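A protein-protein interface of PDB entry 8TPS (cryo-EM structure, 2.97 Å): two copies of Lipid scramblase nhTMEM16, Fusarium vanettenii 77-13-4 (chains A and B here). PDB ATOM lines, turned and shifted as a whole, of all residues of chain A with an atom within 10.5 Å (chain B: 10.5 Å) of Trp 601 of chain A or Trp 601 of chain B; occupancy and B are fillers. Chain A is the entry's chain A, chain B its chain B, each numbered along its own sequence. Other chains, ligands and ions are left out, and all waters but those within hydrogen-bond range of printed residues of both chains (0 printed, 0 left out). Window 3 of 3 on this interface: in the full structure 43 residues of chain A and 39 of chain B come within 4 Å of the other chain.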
ATOM      1  N   TYR A 219      32.170  13.907  20.937  1.00  0.00           N
ATOM      2  CA  TYR A 219      31.130  13.196  20.201  1.00  0.00           C
ATOM      3  C   TYR A 219      30.106  14.164  19.614  1.00  0.00           C
ATOM      4  O   TYR A 219      29.709  14.028  18.444  1.00  0.00           O
ATOM      5  CB  TYR A 219      30.473  12.184  21.145  1.00  0.00           C
ATOM      6  CG  TYR A 219      29.775  11.019  20.485  1.00  0.00           C
ATOM      7  CD1 TYR A 219      28.491  11.142  19.987  1.00  0.00           C
ATOM      8  CD2 TYR A 219      30.404   9.787  20.373  1.00  0.00           C
ATOM      9  CE1 TYR A 219      27.851  10.075  19.386  1.00  0.00           C
ATOM     10  CE2 TYR A 219      29.775   8.715  19.777  1.00  0.00           C
ATOM     11  CZ  TYR A 219      28.497   8.863  19.284  1.00  0.00           C
ATOM     12  OH  TYR A 219      27.863   7.798  18.688  1.00  0.00           O
ATOM     13  N   SER A 578      33.080   9.238  14.304  1.00  0.00           N
ATOM     14  CA  SER A 578      32.431   8.666  15.476  1.00  0.00           C
ATOM     15  C   SER A 578      33.285   7.565  16.087  1.00  0.00           C
ATOM     16  O   SER A 578      33.518   7.555  17.302  1.00  0.00           O
ATOM     17  CB  SER A 578      31.051   8.131  15.104  1.00  0.00           C
ATOM     18  OG  SER A 578      30.721   6.989  15.875  1.00  0.00           O
ATOM     19  N   TYR A 582      35.154   7.065  19.963  1.00  0.00           N
ATOM     20  CA  TYR A 582      35.144   5.931  20.876  1.00  0.00           C
ATOM     21  C   TYR A 582      36.541   5.367  21.089  1.00  0.00           C
ATOM     22  O   TYR A 582      36.859   4.912  22.194  1.00  0.00           O
ATOM     23  CB  TYR A 582      34.210   4.837  20.360  1.00  0.00           C
ATOM     24  CG  TYR A 582      33.958   3.738  21.367  1.00  0.00           C
ATOM     25  CD1 TYR A 582      32.966   3.867  22.328  1.00  0.00           C
ATOM     26  CD2 TYR A 582      34.721   2.578  21.366  1.00  0.00           C
ATOM     27  CE1 TYR A 582      32.733   2.870  23.254  1.00  0.00           C
ATOM     28  CE2 TYR A 582      34.495   1.574  22.289  1.00  0.00           C
ATOM     29  CZ  TYR A 582      33.500   1.726  23.230  1.00  0.00           C
ATOM     30  OH  TYR A 582      33.271   0.730  24.152  1.00  0.00           O
ATOM     31  N   LEU A 583      37.385   5.386  20.058  1.00  0.00           N
ATOM     32  CA  LEU A 583      38.692   4.747  20.147  1.00  0.00           C
ATOM     33  C   LEU A 583      39.710   5.568  20.923  1.00  0.00           C
ATOM     34  O   LEU A 583      40.541   4.993  21.636  1.00  0.00           O
ATOM     35  CB  LEU A 583      39.229   4.452  18.744  1.00  0.00           C
ATOM     36  CG  LEU A 583      38.511   3.327  17.997  1.00  0.00           C
ATOM     37  CD1 LEU A 583      39.209   3.016  16.683  1.00  0.00           C
ATOM     38  CD2 LEU A 583      38.415   2.081  18.864  1.00  0.00           C
ATOM     39  N   ASN A 586      39.003   5.943  25.213  1.00  0.00           N
ATOM     40  CA  ASN A 586      39.103   4.821  26.138  1.00  0.00           C
ATOM     41  C   ASN A 586      40.539   4.315  26.234  1.00  0.00           C
ATOM     42  O   ASN A 586      41.077   3.761  25.275  1.00  0.00           O
ATOM     43  CB  ASN A 586      38.172   3.686  25.708  1.00  0.00           C
ATOM     44  CG  ASN A 586      36.712   4.095  25.713  1.00  0.00           C
ATOM     45  OD1 ASN A 586      36.322   5.058  25.053  1.00  0.00           O
ATOM     46  ND2 ASN A 586      35.895   3.362  26.461  1.00  0.00           N
ATOM     47  N   ALA A 600      34.682  -4.002  20.610  1.00  0.00           N
ATOM     48  CA  ALA A 600      33.728  -3.932  21.709  1.00  0.00           C
ATOM     49  C   ALA A 600      32.333  -3.583  21.203  1.00  0.00           C
ATOM     50  O   ALA A 600      32.172  -3.088  20.087  1.00  0.00           O
ATOM     51  CB  ALA A 600      34.185  -2.917  22.746  1.00  0.00           C
ATOM     52  N   TRP A 601      31.326  -3.847  22.033  1.00  0.00           N
ATOM     53  CA  TRP A 601      29.938  -3.567  21.684  1.00  0.00           C
ATOM     54  C   TRP A 601      29.636  -2.074  21.676  1.00  0.00           C
ATOM     55  O   TRP A 601      28.802  -1.613  20.886  1.00  0.00           O
ATOM     56  CB  TRP A 601      29.006  -4.304  22.653  1.00  0.00           C
ATOM     57  CG  TRP A 601      28.614  -3.512  23.861  1.00  0.00           C
ATOM     58  CD1 TRP A 601      29.364  -3.299  24.981  1.00  0.00           C
ATOM     59  CD2 TRP A 601      27.357  -2.866  24.093  1.00  0.00           C
ATOM     60  NE1 TRP A 601      28.663  -2.538  25.884  1.00  0.00           N
ATOM     61  CE2 TRP A 601      27.426  -2.262  25.363  1.00  0.00           C
ATOM     62  CE3 TRP A 601      26.183  -2.731  23.345  1.00  0.00           C
ATOM     63  CZ2 TRP A 601      26.368  -1.534  25.902  1.00  0.00           C
ATOM     64  CZ3 TRP A 601      25.134  -2.011  23.882  1.00  0.00           C
ATOM     65  CH2 TRP A 601      25.233  -1.419  25.147  1.00  0.00           C
ATOM     66  N   GLY A 602      30.309  -1.303  22.534  1.00  0.00           N
ATOM     67  CA  GLY A 602      30.110   0.135  22.545  1.00  0.00           C
ATOM     68  C   GLY A 602      30.548   0.809  21.261  1.00  0.00           C
ATOM     69  O   GLY A 602      29.893   1.742  20.793  1.00  0.00           O
ATOM     70  N   LEU A 603      31.660   0.353  20.678  1.00  0.00           N
ATOM     71  CA  LEU A 603      32.124   0.919  19.415  1.00  0.00           C
ATOM     72  C   LEU A 603      31.109   0.680  18.305  1.00  0.00           C
ATOM     73  O   LEU A 603      30.804   1.584  17.516  1.00  0.00           O
ATOM     74  CB  LEU A 603      33.482   0.321  19.045  1.00  0.00           C
ATOM     75  CG  LEU A 603      33.942   0.472  17.595  1.00  0.00           C
ATOM     76  CD1 LEU A 603      34.362   1.907  17.319  1.00  0.00           C
ATOM     77  CD2 LEU A 603      35.076  -0.492  17.288  1.00  0.00           C
ATOM     78  N   LEU A 604      30.572  -0.540  18.231  1.00  0.00           N
ATOM     79  CA  LEU A 604      29.563  -0.847  17.223  1.00  0.00           C
ATOM     80  C   LEU A 604      28.295  -0.033  17.448  1.00  0.00           C
ATOM     81  O   LEU A 604      27.690   0.461  16.487  1.00  0.00           O
ATOM     82  CB  LEU A 604      29.252  -2.343  17.231  1.00  0.00           C
ATOM     83  CG  LEU A 604      30.417  -3.266  16.867  1.00  0.00           C
ATOM     84  CD1 LEU A 604      29.941  -4.702  16.722  1.00  0.00           C
ATOM     85  CD2 LEU A 604      31.102  -2.792  15.595  1.00  0.00           C
ATOM     86  N   LEU A 605      27.878   0.116  18.709  1.00  0.00           N
ATOM     87  CA  LEU A 605      26.709   0.938  18.999  1.00  0.00           C
ATOM     88  C   LEU A 605      26.929   2.380  18.562  1.00  0.00           C
ATOM     89  O   LEU A 605      26.041   2.992  17.959  1.00  0.00           O
ATOM     90  CB  LEU A 605      26.374   0.882  20.489  1.00  0.00           C
ATOM     91  CG  LEU A 605      25.019   1.479  20.890  1.00  0.00           C
ATOM     92  CD1 LEU A 605      23.955   1.215  19.829  1.00  0.00           C
ATOM     93  CD2 LEU A 605      24.569   0.972  22.248  1.00  0.00           C
ATOM     94  N   SER A 606      28.105   2.937  18.856  1.00  0.00           N
ATOM     95  CA  SER A 606      28.398   4.310  18.456  1.00  0.00           C
ATOM     96  C   SER A 606      28.400   4.456  16.940  1.00  0.00           C
ATOM     97  O   SER A 606      27.840   5.419  16.404  1.00  0.00           O
ATOM     98  CB  SER A 606      29.738   4.751  19.040  1.00  0.00           C
ATOM     99  OG  SER A 606      30.200   5.936  18.416  1.00  0.00           O
ATOM    100  N   ILE A 607      29.015   3.504  16.232  1.00  0.00           N
ATOM    101  CA  ILE A 607      29.080   3.583  14.775  1.00  0.00           C
ATOM    102  C   ILE A 607      27.679   3.524  14.177  1.00  0.00           C
ATOM    103  O   ILE A 607      27.319   4.330  13.308  1.00  0.00           O
ATOM    104  CB  ILE A 607      29.977   2.465  14.215  1.00  0.00           C
ATOM    105  CG1 ILE A 607      31.451   2.780  14.476  1.00  0.00           C
ATOM    106  CG2 ILE A 607      29.729   2.273  12.727  1.00  0.00           C
ATOM    107  CD1 ILE A 607      32.366   1.591  14.279  1.00  0.00           C
ATOM    108  N   LEU A 608      26.864   2.571  14.639  1.00  0.00           N
ATOM    109  CA  LEU A 608      25.514   2.436  14.105  1.00  0.00           C
ATOM    110  C   LEU A 608      24.646   3.641  14.442  1.00  0.00           C
ATOM    111  O   LEU A 608      23.879   4.099  13.588  1.00  0.00           O
ATOM    112  CB  LEU A 608      24.884   1.129  14.608  1.00  0.00           C
ATOM    113  CG  LEU A 608      24.185   0.985  15.966  1.00  0.00           C
ATOM    114  CD1 LEU A 608      22.738   1.478  15.947  1.00  0.00           C
ATOM    115  CD2 LEU A 608      24.252  -0.460  16.433  1.00  0.00           C
ATOM    116  N   PHE A 609      24.759   4.174  15.662  1.00  0.00           N
ATOM    117  CA  PHE A 609      23.980   5.351  16.027  1.00  0.00           C
ATOM    118  C   PHE A 609      24.378   6.555  15.188  1.00  0.00           C
ATOM    119  O   PHE A 609      23.512   7.310  14.732  1.00  0.00           O
ATOM    120  CB  PHE A 609      24.146   5.656  17.515  1.00  0.00           C
ATOM    121  CG  PHE A 609      23.691   7.034  17.902  1.00  0.00           C
ATOM    122  CD1 PHE A 609      22.346   7.364  17.884  1.00  0.00           C
ATOM    123  CD2 PHE A 609      24.608   8.000  18.282  1.00  0.00           C
ATOM    124  CE1 PHE A 609      21.924   8.631  18.238  1.00  0.00           C
ATOM    125  CE2 PHE A 609      24.192   9.269  18.637  1.00  0.00           C
ATOM    126  CZ  PHE A 609      22.848   9.585  18.615  1.00  0.00           C
ATOM    127  N   TYR B 219      20.672 -17.629   8.430  1.00  0.00           N
ATOM    128  CA  TYR B 219      21.234 -16.323   8.100  1.00  0.00           C
ATOM    129  C   TYR B 219      21.308 -16.118   6.588  1.00  0.00           C
ATOM    130  O   TYR B 219      20.949 -15.042   6.082  1.00  0.00           O
ATOM    131  CB  TYR B 219      22.614 -16.211   8.754  1.00  0.00           C
ATOM    132  CG  TYR B 219      23.123 -14.809   8.987  1.00  0.00           C
ATOM    133  CD1 TYR B 219      23.726 -14.087   7.973  1.00  0.00           C
ATOM    134  CD2 TYR B 219      23.011 -14.213  10.235  1.00  0.00           C
ATOM    135  CE1 TYR B 219      24.196 -12.806   8.187  1.00  0.00           C
ATOM    136  CE2 TYR B 219      23.477 -12.934  10.462  1.00  0.00           C
ATOM    137  CZ  TYR B 219      24.070 -12.233   9.433  1.00  0.00           C
ATOM    138  OH  TYR B 219      24.537 -10.958   9.652  1.00  0.00           O
ATOM    139  N   SER B 578      17.636 -10.288  10.311  1.00  0.00           N
ATOM    140  CA  SER B 578      18.999 -10.606  10.717  1.00  0.00           C
ATOM    141  C   SER B 578      19.106 -10.695  12.231  1.00  0.00           C
ATOM    142  O   SER B 578      19.661 -11.665  12.764  1.00  0.00           O
ATOM    143  CB  SER B 578      19.966  -9.559  10.170  1.00  0.00           C
ATOM    144  OG  SER B 578      21.049  -9.351  11.061  1.00  0.00           O
ATOM    145  N   TYR B 582      20.210 -13.887  14.946  1.00  0.00           N
ATOM    146  CA  TYR B 582      21.140 -13.894  16.064  1.00  0.00           C
ATOM    147  C   TYR B 582      20.435 -14.184  17.382  1.00  0.00           C
ATOM    148  O   TYR B 582      21.012 -14.839  18.257  1.00  0.00           O
ATOM    149  CB  TYR B 582      21.884 -12.561  16.151  1.00  0.00           C
ATOM    150  CG  TYR B 582      23.035 -12.578  17.131  1.00  0.00           C
ATOM    151  CD1 TYR B 582      24.288 -13.036  16.748  1.00  0.00           C
ATOM    152  CD2 TYR B 582      22.867 -12.150  18.440  1.00  0.00           C
ATOM    153  CE1 TYR B 582      25.344 -13.059  17.638  1.00  0.00           C
ATOM    154  CE2 TYR B 582      23.918 -12.170  19.338  1.00  0.00           C
ATOM    155  CZ  TYR B 582      25.153 -12.626  18.932  1.00  0.00           C
ATOM    156  OH  TYR B 582      26.202 -12.648  19.821  1.00  0.00           O
ATOM    157  N   LEU B 583      19.199 -13.712  17.544  1.00  0.00           N
ATOM    158  CA  LEU B 583      18.511 -13.836  18.823  1.00  0.00           C
ATOM    159  C   LEU B 583      17.952 -15.228  19.071  1.00  0.00           C
ATOM    160  O   LEU B 583      17.961 -15.693  20.216  1.00  0.00           O
ATOM    161  CB  LEU B 583      17.384 -12.804  18.915  1.00  0.00           C
ATOM    162  CG  LEU B 583      17.844 -11.353  19.080  1.00  0.00           C
ATOM    163  CD1 LEU B 583      16.658 -10.432  19.308  1.00  0.00           C
ATOM    164  CD2 LEU B 583      18.848 -11.233  20.216  1.00  0.00           C
ATOM    165  N   ASN B 586      20.890 -18.386  19.734  1.00  0.00           N
ATOM    166  CA  ASN B 586      21.744 -18.445  20.914  1.00  0.00           C
ATOM    167  C   ASN B 586      20.920 -18.695  22.174  1.00  0.00           C
ATOM    168  O   ASN B 586      20.144 -17.840  22.599  1.00  0.00           O
ATOM    169  CB  ASN B 586      22.550 -17.153  21.059  1.00  0.00           C
ATOM    170  CG  ASN B 586      23.482 -16.913  19.889  1.00  0.00           C
ATOM    171  OD1 ASN B 586      23.053 -16.861  18.737  1.00  0.00           O
ATOM    172  ND2 ASN B 586      24.770 -16.766  20.179  1.00  0.00           N
ATOM    173  N   ALA B 600      24.657  -7.722  23.028  1.00  0.00           N
ATOM    174  CA  ALA B 600      25.984  -8.260  22.756  1.00  0.00           C
ATOM    175  C   ALA B 600      26.585  -7.628  21.506  1.00  0.00           C
ATOM    176  O   ALA B 600      25.875  -7.039  20.691  1.00  0.00           O
ATOM    177  CB  ALA B 600      25.924  -9.773  22.610  1.00  0.00           C
ATOM    178  N   TRP B 601      27.904  -7.754  21.364  1.00  0.00           N
ATOM    179  CA  TRP B 601      28.618  -7.200  20.219  1.00  0.00           C
ATOM    180  C   TRP B 601      28.332  -7.969  18.936  1.00  0.00           C
ATOM    181  O   TRP B 601      28.317  -7.378  17.847  1.00  0.00           O
ATOM    182  CB  TRP B 601      30.120  -7.175  20.514  1.00  0.00           C
ATOM    183  CG  TRP B 601      30.859  -8.403  20.079  1.00  0.00           C
ATOM    184  CD1 TRP B 601      30.903  -9.604  20.724  1.00  0.00           C
ATOM    185  CD2 TRP B 601      31.699  -8.537  18.927  1.00  0.00           C
ATOM    186  NE1 TRP B 601      31.697 -10.485  20.032  1.00  0.00           N
ATOM    187  CE2 TRP B 601      32.200  -9.853  18.925  1.00  0.00           C
ATOM    188  CE3 TRP B 601      32.067  -7.674  17.889  1.00  0.00           C
ATOM    189  CZ2 TRP B 601      33.049 -10.328  17.928  1.00  0.00           C
ATOM    190  CZ3 TRP B 601      32.912  -8.147  16.903  1.00  0.00           C
ATOM    191  CH2 TRP B 601      33.392  -9.462  16.928  1.00  0.00           C
ATOM    192  N   GLY B 602      28.090  -9.278  19.041  1.00  0.00           N
ATOM    193  CA  GLY B 602      27.759 -10.063  17.865  1.00  0.00           C
ATOM    194  C   GLY B 602      26.450  -9.654  17.223  1.00  0.00           C
ATOM    195  O   GLY B 602      26.337  -9.637  15.995  1.00  0.00           O
ATOM    196  N   LEU B 603      25.443  -9.324  18.037  1.00  0.00           N
ATOM    197  CA  LEU B 603      24.164  -8.876  17.495  1.00  0.00           C
ATOM    198  C   LEU B 603      24.328  -7.578  16.714  1.00  0.00           C
ATOM    199  O   LEU B 603      23.779  -7.424  15.616  1.00  0.00           O
ATOM    200  CB  LEU B 603      23.153  -8.700  18.629  1.00  0.00           C
ATOM    201  CG  LEU B 603      21.905  -7.869  18.332  1.00  0.00           C
ATOM    202  CD1 LEU B 603      20.951  -8.645  17.437  1.00  0.00           C
ATOM    203  CD2 LEU B 603      21.217  -7.453  19.622  1.00  0.00           C
ATOM    204  N   LEU B 604      25.086  -6.630  17.269  1.00  0.00           N
ATOM    205  CA  LEU B 604      25.328  -5.372  16.575  1.00  0.00           C
ATOM    206  C   LEU B 604      26.116  -5.595  15.290  1.00  0.00           C
ATOM    207  O   LEU B 604      25.821  -4.974  14.260  1.00  0.00           O
ATOM    208  CB  LEU B 604      26.063  -4.397  17.495  1.00  0.00           C
ATOM    209  CG  LEU B 604      25.306  -3.973  18.754  1.00  0.00           C
ATOM    210  CD1 LEU B 604      26.050  -2.867  19.483  1.00  0.00           C
ATOM    211  CD2 LEU B 604      23.890  -3.537  18.411  1.00  0.00           C
ATOM    212  N   LEU B 605      27.120  -6.476  15.331  1.00  0.00           N
ATOM    213  CA  LEU B 605      27.870  -6.785  14.120  1.00  0.00           C
ATOM    214  C   LEU B 605      26.965  -7.381  13.049  1.00  0.00           C
ATOM    215  O   LEU B 605      27.051  -6.999  11.877  1.00  0.00           O
ATOM    216  CB  LEU B 605      29.018  -7.744  14.434  1.00  0.00           C
ATOM    217  CG  LEU B 605      30.046  -7.941  13.312  1.00  0.00           C
ATOM    218  CD1 LEU B 605      30.283  -6.650  12.536  1.00  0.00           C
ATOM    219  CD2 LEU B 605      31.352  -8.499  13.848  1.00  0.00           C
ATOM    220  N   SER B 606      26.093  -8.315  13.433  1.00  0.00           N
ATOM    221  CA  SER B 606      25.180  -8.919  12.468  1.00  0.00           C
ATOM    222  C   SER B 606      24.229  -7.885  11.881  1.00  0.00           C
ATOM    223  O   SER B 606      23.996  -7.867  10.667  1.00  0.00           O
ATOM    224  CB  SER B 606      24.398 -10.054  13.128  1.00  0.00           C
ATOM    225  OG  SER B 606      23.293 -10.441  12.332  1.00  0.00           O
ATOM    226  N   ILE B 607      23.679  -7.008  12.726  1.00  0.00           N
ATOM    227  CA  ILE B 607      22.740  -5.998  12.243  1.00  0.00           C
ATOM    228  C   ILE B 607      23.429  -5.057  11.261  1.00  0.00           C
ATOM    229  O   ILE B 607      22.905  -4.768  10.177  1.00  0.00           O
ATOM    230  CB  ILE B 607      22.126  -5.225  13.425  1.00  0.00           C
ATOM    231  CG1 ILE B 607      21.099  -6.091  14.155  1.00  0.00           C
ATOM    232  CG2 ILE B 607      21.489  -3.930  12.947  1.00  0.00           C
ATOM    233  CD1 ILE B 607      20.712  -5.552  15.515  1.00  0.00           C
ATOM    234  N   LEU B 608      24.618  -4.570  11.624  1.00  0.00           N
ATOM    235  CA  LEU B 608      25.334  -3.649  10.750  1.00  0.00           C
ATOM    236  C   LEU B 608      25.764  -4.317   9.451  1.00  0.00           C
ATOM    237  O   LEU B 608      25.663  -3.700   8.384  1.00  0.00           O
ATOM    238  CB  LEU B 608      26.533  -3.046  11.496  1.00  0.00           C
ATOM    239  CG  LEU B 608      27.898  -3.734  11.616  1.00  0.00           C
ATOM    240  CD1 LEU B 608      28.780  -3.530  10.385  1.00  0.00           C
ATOM    241  CD2 LEU B 608      28.612  -3.255  12.871  1.00  0.00           C
ATOM    242  N   PHE B 609      26.227  -5.569   9.512  1.00  0.00           N
ATOM    243  CA  PHE B 609      26.617  -6.270   8.295  1.00  0.00           C
ATOM    244  C   PHE B 609      25.424  -6.488   7.378  1.00  0.00           C
ATOM    245  O   PHE B 609      25.533  -6.307   6.161  1.00  0.00           O
ATOM    246  CB  PHE B 609      27.277  -7.605   8.642  1.00  0.00           C
ATOM    247  CG  PHE B 609      27.377  -8.548   7.477  1.00  0.00           C
ATOM    248  CD1 PHE B 609      28.239  -8.282   6.426  1.00  0.00           C
ATOM    249  CD2 PHE B 609      26.607  -9.699   7.432  1.00  0.00           C
ATOM    250  CE1 PHE B 609      28.331  -9.147   5.352  1.00  0.00           C
ATOM    251  CE2 PHE B 609      26.697 -10.567   6.361  1.00  0.00           C
ATOM    252  CZ  PHE B 609      27.559 -10.291   5.319  1.00  0.00           C
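Trp 601 of chain A touches Trp 601 of chain B (CB to CB, 3.7 Å). Leu 604 of chain B touches Trp 601 of chain A. O of Trp 601 of chain B touches CD1 of Leu 604 of chain A, at 3.3 Å. Leu 604 of chain B touches Leu 604 of chain A. N of Leu 605 of chain B touches CD1 of Leu 604 of chain A, at 3.6 Å. CD2 of Leu 604 of chain A touches CD2 of Leu 608 of chain B (3.7 Å). Leu 604 of chain B touches Leu 605 of chain A (CD1 to N, 3.6 Å). CD2 of Leu 604 of chain B touches CD2 of Leu 608 of chain A (3.7 Å).
Trp 601 of chain A touches just these residues of chain B: Trp 601 (3.7 Å) and Leu 604 (3.3 Å). Of the printed residues of chain A, Trp 601 of chain B touches Trp 601 and Leu 604. No residue of chain B comes within 4 Å of Ala 600 of chain A. No residue of chain B comes within 4 Å of Gly 602 of chain A. Of the printed residues of chain B, Leu 604 of chain A touches Trp 601 (3.3 Å), Leu 604 (3.8 Å), Leu 605 (3.6 Å) and Leu 608 (3.7 Å). Leu 605 of chain A touches one residue of chain B. No residue of chain A comes within 4 Å of Ala 600 of chain B. No residue of chain A comes within 4 Å of Gly 602 of chain B. Leu 604 of chain B touches four residues of chain A. Of chain A, only Leu 604 comes within 4 Å of Leu 605 of chain B. Of the printed residues of chain B, Leu 608 of chain A touches Leu 604 (3.7 Å). Of the printed residues of chain A, Leu 608 of chain B touches Leu 604. Ile 607 of chain B touches none of the printed residues of chain A. Leu 603 of chain A touches none of the printed residues of chain B. The nearest residue of chain B that does not touch Trp 601 of chain A is Ala 600 of chain B (4.3 Å). The nearest printed residue of chain B that does not touch Leu 608 of chain A is Leu 608 of chain B (5.5 Å).
Of the 15 printed residues of chain A, 4 touch a printed residue of chain B. Hydrophobic or aromatic side chains of chain A within 4 Å of the printed part of chain B: Trp 601, Leu 604, Leu 605 and Leu 608. Hydrophobic or aromatic side chains of chain B that line the printed part of chain A: Trp 601, Leu 604, Leu 605 and Leu 608. Among the printed residues, no Asp or Glu carboxylate lies within 4 Å of a Lys or Arg side-chain nitrogen of the other chain.
Trp 601 of chain B touches its own counterpart, Trp 601 of chain A. Trp 601 of chain A touches Leu 604 of chain B, and with the chains exchanged Leu 604 of chain A touches Trp 601 of chain B. Leu 604 of chain A touches its own counterpart, Leu 604 of chain B. Leu 604 of chain A touches Leu 605 of chain B, and with the chains exchanged Leu 605 of chain A touches Leu 604 of chain B. Of the 8 pairs that touch across the chains among the printed residues, 8 have their exchanged pair printed and touching as well.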
